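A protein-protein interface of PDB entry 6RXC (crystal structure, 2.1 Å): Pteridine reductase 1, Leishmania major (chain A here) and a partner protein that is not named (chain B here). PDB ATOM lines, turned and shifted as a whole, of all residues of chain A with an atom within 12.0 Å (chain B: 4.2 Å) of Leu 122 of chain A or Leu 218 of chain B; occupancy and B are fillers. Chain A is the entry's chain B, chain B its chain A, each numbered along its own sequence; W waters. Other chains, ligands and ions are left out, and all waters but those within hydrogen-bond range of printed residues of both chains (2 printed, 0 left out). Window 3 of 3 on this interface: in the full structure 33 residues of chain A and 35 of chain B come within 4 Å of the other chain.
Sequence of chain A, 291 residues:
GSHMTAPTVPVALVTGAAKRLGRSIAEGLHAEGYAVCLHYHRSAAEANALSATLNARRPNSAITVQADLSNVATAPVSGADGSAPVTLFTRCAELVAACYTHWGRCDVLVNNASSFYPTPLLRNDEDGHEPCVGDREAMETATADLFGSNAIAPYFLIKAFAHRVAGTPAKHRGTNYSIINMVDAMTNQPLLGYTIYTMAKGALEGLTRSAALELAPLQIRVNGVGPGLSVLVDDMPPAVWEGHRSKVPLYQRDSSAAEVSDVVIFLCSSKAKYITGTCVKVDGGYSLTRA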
ATOM      1  N   PRO A 118      23.371   5.370 -11.694  1.00  0.00           N
ATOM      2  CA  PRO A 118      23.020   6.731 -11.308  1.00  0.00           C
ATOM      3  C   PRO A 118      21.521   6.872 -11.119  1.00  0.00           C
ATOM      4  O   PRO A 118      20.757   6.304 -11.894  1.00  0.00           O
ATOM      5  CB  PRO A 118      23.250   7.590 -12.572  1.00  0.00           C
ATOM      6  CG  PRO A 118      24.149   6.756 -13.468  1.00  0.00           C
ATOM      7  CD  PRO A 118      23.988   5.316 -13.035  1.00  0.00           C
ATOM      8  N   THR A 119      21.130   7.638 -10.080  1.00  0.00           N
ATOM      9  CA  THR A 119      19.778   8.122  -9.966  1.00  0.00           C
ATOM     10  C   THR A 119      19.891   9.597  -9.638  1.00  0.00           C
ATOM     11  O   THR A 119      19.753   9.968  -8.454  1.00  0.00           O
ATOM     12  CB  THR A 119      19.091   7.446  -8.784  1.00  0.00           C
ATOM     13  OG1 THR A 119      19.987   7.505  -7.659  1.00  0.00           O
ATOM     14  CG2 THR A 119      18.757   6.007  -9.116  1.00  0.00           C
ATOM     15  N   PRO A 120      20.104  10.453 -10.660  1.00  0.00           N
ATOM     16  CA  PRO A 120      20.503  11.838 -10.405  1.00  0.00           C
ATOM     17  C   PRO A 120      19.318  12.641  -9.882  1.00  0.00           C
ATOM     18  O   PRO A 120      18.176  12.322 -10.211  1.00  0.00           O
ATOM     19  CB  PRO A 120      20.915  12.375 -11.790  1.00  0.00           C
ATOM     20  CG  PRO A 120      20.977  11.105 -12.650  1.00  0.00           C
ATOM     21  CD  PRO A 120      19.908  10.183 -12.095  1.00  0.00           C
ATOM     22  N   LEU A 121      19.626  13.717  -9.140  1.00  0.00           N
ATOM     23  CA  LEU A 121      18.636  14.672  -8.684  1.00  0.00           C
ATOM     24  C   LEU A 121      18.389  15.758  -9.729  1.00  0.00           C
ATOM     25  O   LEU A 121      17.246  16.130  -9.941  1.00  0.00           O
ATOM     26  CB  LEU A 121      19.007  15.239  -7.300  1.00  0.00           C
ATOM     27  CG  LEU A 121      19.110  14.233  -6.165  1.00  0.00           C
ATOM     28  CD1 LEU A 121      19.944  14.813  -5.040  1.00  0.00           C
ATOM     29  CD2 LEU A 121      17.746  13.712  -5.689  1.00  0.00           C
ATOM     30  N   LEU A 122      19.411  16.300 -10.387  1.00  0.00           N
ATOM     31  CA  LEU A 122      19.080  17.308 -11.406  1.00  0.00           C
ATOM     32  C   LEU A 122      19.223  16.738 -12.820  1.00  0.00           C
ATOM     33  O   LEU A 122      19.386  15.537 -12.951  1.00  0.00           O
ATOM     34  CB  LEU A 122      19.947  18.560 -11.262  1.00  0.00           C
ATOM     35  CG  LEU A 122      20.199  19.040  -9.839  1.00  0.00           C
ATOM     36  CD1 LEU A 122      21.377  20.006  -9.802  1.00  0.00           C
ATOM     37  CD2 LEU A 122      18.928  19.657  -9.246  1.00  0.00           C
ATOM     38  N   ARG A 123      19.121  17.610 -13.851  1.00  0.00           N
ATOM     39  CA  ARG A 123      19.367  17.337 -15.274  1.00  0.00           C
ATOM     40  C   ARG A 123      18.444  16.220 -15.775  1.00  0.00           C
ATOM     41  O   ARG A 123      17.374  16.023 -15.197  1.00  0.00           O
ATOM     42  CB  ARG A 123      20.861  17.095 -15.554  1.00  0.00           C
ATOM     43  CG  ARG A 123      21.761  18.312 -15.353  1.00  0.00           C
ATOM     44  CD  ARG A 123      22.323  18.930 -16.623  1.00  0.00           C
ATOM     45  NE  ARG A 123      21.392  19.525 -17.587  1.00  0.00           N
ATOM     46  CZ  ARG A 123      20.247  20.153 -17.309  1.00  0.00           C
ATOM     47  NH1 ARG A 123      19.846  20.298 -16.054  1.00  0.00           N
ATOM     48  NH2 ARG A 123      19.504  20.631 -18.295  1.00  0.00           N
ATOM     49  N   ASN A 124      18.843  15.505 -16.850  1.00  0.00           N
ATOM     50  CA  ASN A 124      18.184  14.266 -17.256  1.00  0.00           C
ATOM     51  C   ASN A 124      19.164  13.358 -18.014  1.00  0.00           C
ATOM     52  O   ASN A 124      19.266  12.155 -17.634  1.00  0.00           O
ATOM     53  CB  ASN A 124      16.879  14.500 -18.023  1.00  0.00           C
ATOM     54  N   ALA A 138      11.461   4.733 -15.411  1.00  0.00           N
ATOM     55  CA  ALA A 138      12.784   4.492 -14.871  1.00  0.00           C
ATOM     56  C   ALA A 138      12.726   4.506 -13.333  1.00  0.00           C
ATOM     57  O   ALA A 138      13.023   3.503 -12.681  1.00  0.00           O
ATOM     58  CB  ALA A 138      13.769   5.483 -15.464  1.00  0.00           C
ATOM     59  N   MET A 139      12.249   5.619 -12.770  1.00  0.00           N
ATOM     60  CA  MET A 139      12.404   5.896 -11.354  1.00  0.00           C
ATOM     61  C   MET A 139      11.799   4.809 -10.473  1.00  0.00           C
ATOM     62  O   MET A 139      12.446   4.405  -9.501  1.00  0.00           O
ATOM     63  CB  MET A 139      11.945   7.301 -10.948  1.00  0.00           C
ATOM     64  CG  MET A 139      13.077   8.323 -11.029  1.00  0.00           C
ATOM     65  SD  MET A 139      14.238   8.192  -9.620  1.00  0.00           S
ATOM     66  CE  MET A 139      15.285   9.616  -9.932  1.00  0.00           C
ATOM     67  N   LEU A 191      29.340   9.430  -4.360  1.00  0.00           N
ATOM     68  CA  LEU A 191      29.518   9.514  -5.786  1.00  0.00           C
ATOM     69  C   LEU A 191      28.386  10.367  -6.325  1.00  0.00           C
ATOM     70  O   LEU A 191      27.214  10.083  -6.046  1.00  0.00           O
ATOM     71  CB  LEU A 191      29.353   8.053  -6.226  1.00  0.00           C
ATOM     72  CG  LEU A 191      29.918   7.621  -7.577  1.00  0.00           C
ATOM     73  CD1 LEU A 191      31.399   7.983  -7.730  1.00  0.00           C
ATOM     74  CD2 LEU A 191      29.725   6.112  -7.690  1.00  0.00           C
ATOM     75  N   LEU A 192      28.743  11.402  -7.076  1.00  0.00           N
ATOM     76  CA  LEU A 192      27.777  12.380  -7.548  1.00  0.00           C
ATOM     77  C   LEU A 192      26.778  11.683  -8.473  1.00  0.00           C
ATOM     78  O   LEU A 192      27.210  11.030  -9.420  1.00  0.00           O
ATOM     79  CB  LEU A 192      28.553  13.465  -8.303  1.00  0.00           C
ATOM     80  CG  LEU A 192      27.832  14.806  -8.481  1.00  0.00           C
ATOM     81  CD1 LEU A 192      27.881  15.626  -7.184  1.00  0.00           C
ATOM     82  CD2 LEU A 192      28.416  15.628  -9.629  1.00  0.00           C
ATOM     83  N   GLY A 193      25.464  11.829  -8.202  1.00  0.00           N
ATOM     84  CA  GLY A 193      24.443  11.271  -9.078  1.00  0.00           C
ATOM     85  C   GLY A 193      24.062   9.831  -8.700  1.00  0.00           C
ATOM     86  O   GLY A 193      23.362   9.172  -9.478  1.00  0.00           O
ATOM     87  N   TYR A 194      24.450   9.353  -7.505  1.00  0.00           N
ATOM     88  CA  TYR A 194      24.218   7.983  -7.099  1.00  0.00           C
ATOM     89  C   TYR A 194      23.395   7.863  -5.805  1.00  0.00           C
ATOM     90  O   TYR A 194      23.630   6.943  -4.997  1.00  0.00           O
ATOM     91  CB  TYR A 194      25.508   7.169  -7.123  1.00  0.00           C
ATOM     92  CG  TYR A 194      26.081   6.816  -8.481  1.00  0.00           C
ATOM     93  CD1 TYR A 194      26.853   7.718  -9.216  1.00  0.00           C
ATOM     94  CD2 TYR A 194      25.862   5.555  -9.027  1.00  0.00           C
ATOM     95  CE1 TYR A 194      27.406   7.381 -10.442  1.00  0.00           C
ATOM     96  CE2 TYR A 194      26.386   5.217 -10.268  1.00  0.00           C
ATOM     97  CZ  TYR A 194      27.161   6.125 -10.964  1.00  0.00           C
ATOM     98  OH  TYR A 194      27.714   5.746 -12.147  1.00  0.00           O
ATOM     99  N   THR A 195      22.532   8.846  -5.495  1.00  0.00           N
ATOM    100  CA  THR A 195      21.845   8.877  -4.159  1.00  0.00           C
ATOM    101  C   THR A 195      21.168   7.564  -3.766  1.00  0.00           C
ATOM    102  O   THR A 195      21.393   7.129  -2.619  1.00  0.00           O
ATOM    103  CB  THR A 195      20.756   9.944  -3.992  1.00  0.00           C
ATOM    104  OG1 THR A 195      21.330  11.215  -4.299  1.00  0.00           O
ATOM    105  CG2 THR A 195      20.166   9.971  -2.598  1.00  0.00           C
ATOM    106  N   ILE A 196      20.316   7.027  -4.648  1.00  0.00           N
ATOM    107  CA  ILE A 196      19.577   5.755  -4.380  1.00  0.00           C
ATOM    108  C   ILE A 196      20.586   4.718  -3.880  1.00  0.00           C
ATOM    109  O   ILE A 196      20.403   4.201  -2.760  1.00  0.00           O
ATOM    110  CB  ILE A 196      18.839   5.273  -5.644  1.00  0.00           C
ATOM    111  CG1 ILE A 196      17.902   6.350  -6.200  1.00  0.00           C
ATOM    112  CG2 ILE A 196      18.103   3.969  -5.376  1.00  0.00           C
ATOM    113  CD1 ILE A 196      16.439   6.091  -5.930  1.00  0.00           C
ATOM    114  N   ALA B 162      14.257  20.080  -5.400  1.00  0.00           N
ATOM    115  CA  ALA B 162      15.399  20.439  -6.229  1.00  0.00           C
ATOM    116  C   ALA B 162      14.955  20.902  -7.611  1.00  0.00           C
ATOM    117  O   ALA B 162      15.517  21.848  -8.171  1.00  0.00           O
ATOM    118  CB  ALA B 162      16.307  19.242  -6.347  1.00  0.00           C
ATOM    119  N   VAL B 165      13.563  24.480  -7.694  1.00  0.00           N
ATOM    120  CA  VAL B 165      14.593  25.516  -7.652  1.00  0.00           C
ATOM    121  C   VAL B 165      15.300  25.602  -9.003  1.00  0.00           C
ATOM    122  O   VAL B 165      15.436  26.680  -9.593  1.00  0.00           O
ATOM    123  CB  VAL B 165      15.624  25.236  -6.537  1.00  0.00           C
ATOM    124  CG1 VAL B 165      16.856  26.180  -6.625  1.00  0.00           C
ATOM    125  CG2 VAL B 165      14.929  25.330  -5.171  1.00  0.00           C
ATOM    126  N   ALA B 166      15.759  24.451  -9.487  1.00  0.00           N
ATOM    127  CA  ALA B 166      16.454  24.378 -10.748  1.00  0.00           C
ATOM    128  C   ALA B 166      15.588  24.980 -11.847  1.00  0.00           C
ATOM    129  O   ALA B 166      16.118  25.560 -12.802  1.00  0.00           O
ATOM    130  CB  ALA B 166      16.786  22.937 -10.993  1.00  0.00           C
ATOM    131  N   ARG B 173      15.392  33.221  -7.641  1.00  0.00           N
ATOM    132  CA  ARG B 173      15.553  32.147  -6.668  1.00  0.00           C
ATOM    133  C   ARG B 173      15.616  32.718  -5.255  1.00  0.00           C
ATOM    134  O   ARG B 173      16.133  33.824  -5.069  1.00  0.00           O
ATOM    135  CB  ARG B 173      16.789  31.303  -7.005  1.00  0.00           C
ATOM    136  CG  ARG B 173      16.513  30.189  -8.010  1.00  0.00           C
ATOM    137  CD  ARG B 173      17.816  29.550  -8.457  1.00  0.00           C
ATOM    138  NE  ARG B 173      17.626  28.922  -9.790  1.00  0.00           N
ATOM    139  CZ  ARG B 173      18.540  28.312 -10.516  1.00  0.00           C
ATOM    140  NH1 ARG B 173      19.787  28.272 -10.101  1.00  0.00           N
ATOM    141  NH2 ARG B 173      18.210  27.781 -11.684  1.00  0.00           N
ATOM    142  N   GLU B 214      25.296  16.956  -4.332  1.00  0.00           N
ATOM    143  CA  GLU B 214      24.799  17.213  -5.670  1.00  0.00           C
ATOM    144  C   GLU B 214      24.013  18.525  -5.730  1.00  0.00           C
ATOM    145  O   GLU B 214      23.966  19.175  -6.767  1.00  0.00           O
ATOM    146  CB  GLU B 214      23.917  16.030  -6.101  1.00  0.00           C
ATOM    147  CG  GLU B 214      23.426  16.090  -7.547  1.00  0.00           C
ATOM    148  CD  GLU B 214      22.641  14.891  -8.078  1.00  0.00           C
ATOM    149  OE1 GLU B 214      22.476  13.868  -7.351  1.00  0.00           O
ATOM    150  OE2 GLU B 214      22.165  14.980  -9.186  1.00  0.00           O
ATOM    151  N   LEU B 215      23.409  18.959  -4.619  1.00  0.00           N
ATOM    152  CA  LEU B 215      22.630  20.196  -4.666  1.00  0.00           C
ATOM    153  C   LEU B 215      23.406  21.430  -4.185  1.00  0.00           C
ATOM    154  O   LEU B 215      22.825  22.539  -4.101  1.00  0.00           O
ATOM    155  CB  LEU B 215      21.385  20.035  -3.778  1.00  0.00           C
ATOM    156  CG  LEU B 215      20.481  18.845  -4.071  1.00  0.00           C
ATOM    157  CD1 LEU B 215      19.354  18.854  -3.067  1.00  0.00           C
ATOM    158  CD2 LEU B 215      20.004  18.936  -5.495  1.00  0.00           C
ATOM    159  N   ALA B 216      24.660  21.242  -3.728  1.00  0.00           N
ATOM    160  CA  ALA B 216      25.498  22.388  -3.447  1.00  0.00           C
ATOM    161  C   ALA B 216      25.554  23.394  -4.626  1.00  0.00           C
ATOM    162  O   ALA B 216      25.680  24.601  -4.420  1.00  0.00           O
ATOM    163  CB  ALA B 216      26.896  21.892  -3.161  1.00  0.00           C
ATOM    164  N   PRO B 217      25.542  23.018  -5.916  1.00  0.00           N
ATOM    165  CA  PRO B 217      25.617  24.045  -6.956  1.00  0.00           C
ATOM    166  C   PRO B 217      24.415  24.980  -6.999  1.00  0.00           C
ATOM    167  O   PRO B 217      24.556  26.067  -7.502  1.00  0.00           O
ATOM    168  CB  PRO B 217      25.747  23.249  -8.268  1.00  0.00           C
ATOM    169  CG  PRO B 217      26.371  21.911  -7.792  1.00  0.00           C
ATOM    170  CD  PRO B 217      25.675  21.654  -6.466  1.00  0.00           C
ATOM    171  N   LEU B 218      23.241  24.525  -6.535  1.00  0.00           N
ATOM    172  CA  LEU B 218      22.106  25.412  -6.378  1.00  0.00           C
ATOM    173  C   LEU B 218      22.010  26.028  -4.978  1.00  0.00           C
ATOM    174  O   LEU B 218      20.935  26.526  -4.617  1.00  0.00           O
ATOM    175  CB  LEU B 218      20.852  24.549  -6.584  1.00  0.00           C
ATOM    176  CG  LEU B 218      20.575  24.063  -7.998  1.00  0.00           C
ATOM    177  CD1 LEU B 218      19.393  23.062  -7.928  1.00  0.00           C
ATOM    178  CD2 LEU B 218      20.228  25.272  -8.877  1.00  0.00           C
ATOM    179  N   GLN B 219      23.064  25.930  -4.157  1.00  0.00           N
ATOM    180  CA  GLN B 219      23.075  26.532  -2.826  1.00  0.00           C
ATOM    181  C   GLN B 219      21.934  25.949  -1.977  1.00  0.00           C
ATOM    182  O   GLN B 219      21.359  26.626  -1.137  1.00  0.00           O
ATOM    183  CB  GLN B 219      23.058  28.073  -2.864  1.00  0.00           C
ATOM    184  CG  GLN B 219      24.077  28.666  -3.817  1.00  0.00           C
ATOM    185  CD  GLN B 219      24.281  30.146  -3.606  1.00  0.00           C
ATOM    186  OE1 GLN B 219      23.497  30.837  -2.958  1.00  0.00           O
ATOM    187  NE2 GLN B 219      25.358  30.646  -4.162  1.00  0.00           N
ATOM    188  N   ILE B 220      21.601  24.677  -2.211  1.00  0.00           N
ATOM    189  CA  ILE B 220      20.629  24.032  -1.362  1.00  0.00           C
ATOM    190  C   ILE B 220      21.454  23.244  -0.376  1.00  0.00           C
ATOM    191  O   ILE B 220      22.216  22.342  -0.775  1.00  0.00           O
ATOM    192  CB  ILE B 220      19.689  23.126  -2.182  1.00  0.00           C
ATOM    193  CG1 ILE B 220      18.935  23.917  -3.268  1.00  0.00           C
ATOM    194  CG2 ILE B 220      18.782  22.304  -1.266  1.00  0.00           C
ATOM    195  CD1 ILE B 220      18.037  23.062  -4.153  1.00  0.00           C
HETATM  196  O   HOH W   1      21.690  11.500  -6.819  1.00  0.00           O
HETATM  197  O   HOH W   2      25.041  12.809  -5.458  1.00  0.00           O
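OE2 of Glu 214 of chain B is in hydrogen-bond range of N of Leu 122 of chain A (3.3 Å).
N of Leu 121 of chain A is in hydrogen-bond range of OE2 of Glu 214 of chain B (2.8 Å).
O of Gly 193 of chain A lies within hydrogen-bond range of N of Thr 119 of chain A (2.8 Å).
N of Ile 220 of chain B sits at hydrogen-bond distance from O of Leu 215 of chain B, 3.1 Å away.
Glu 214 of chain B touches Pro 120 of chain A.
CD2 of Leu 122 of chain A touches CB of Ala 162 of chain B, at 3.9 Å.
Leu 122 of chain A touches Leu 215 of chain B.
CD1 of Leu 218 of chain B touches CD2 of Leu 122 of chain A, 3.7 Å away.
Glu 214 of chain B touches Leu 192 of chain A.
Gly 193 of chain A touches Glu 214 of chain B.
Printed residues of chain B within 4 Å of Pro 120 of chain A: Glu 214 (3.7 Å).
Printed residues of chain B within 4 Å of Leu 121 of chain A: Glu 214 (2.8 Å).
Of chain B, only Ala 162 (3.9 Å), Glu 214 (3.3 Å), Leu 215 (3.97 Å) and Leu 218 (3.7 Å) come within 4 Å of Leu 122 of chain A.
Of the printed residues of chain B, Leu 192 of chain A touches Glu 214 (3.8 Å).
Of the printed residues of chain B, Gly 193 of chain A touches Glu 214 (3.7 Å).
No residue of chain A comes within 4 Å of Val 165 of chain B.
No residue of chain A comes within 4 Å of Ala 166 of chain B.
Of chain A, only Pro 120 (3.7 Å), Leu 121 (2.8 Å), Leu 122 (3.3 Å), Leu 192 (3.8 Å) and Gly 193 (3.7 Å) come within 4 Å of Glu 214 of chain B.
Of chain A, only Leu 122 (3.97 Å) comes within 4 Å of Leu 215 of chain B.
No residue of chain A comes within 4 Å of Pro 217 of chain B.
Printed residues of chain A within 4 Å of Leu 218 of chain B: Leu 122 (3.7 Å).
No residue of chain A comes within 4 Å of Gln 219 of chain B.
No residue of chain A comes within 4 Å of Ile 220 of chain B.
The nearest residue of chain A that does not touch Leu 218 of chain B is Leu 121 of chain A (7.5 Å).
Printed residues of chain B that touch a printed residue of chain A: Ala 162, Glu 214, Leu 215 and Leu 218.
Hydrophobic or aromatic side chains of chain B that line the printed part of chain A: Ala 162, Leu 215 and Leu 218.
Among the printed residues, 8 pairs touch across the chains.
Among the printed residues, no Asp or Glu carboxylate lies within 4 Å of a Lys or Arg side-chain nitrogen of the other chain.
Water W1 lies within hydrogen-bond range of OE1 of Glu 214 of chain B (2.6 Å), OG1 of Thr 195 of chain A (2.6 Å) and O of Thr 119 of chain A (3.0 Å).
Water W2 lies within hydrogen-bond range of N of Gly 193 of chain A (2.9 Å) and OE1 of Glu 214 of chain B (3.4 Å).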
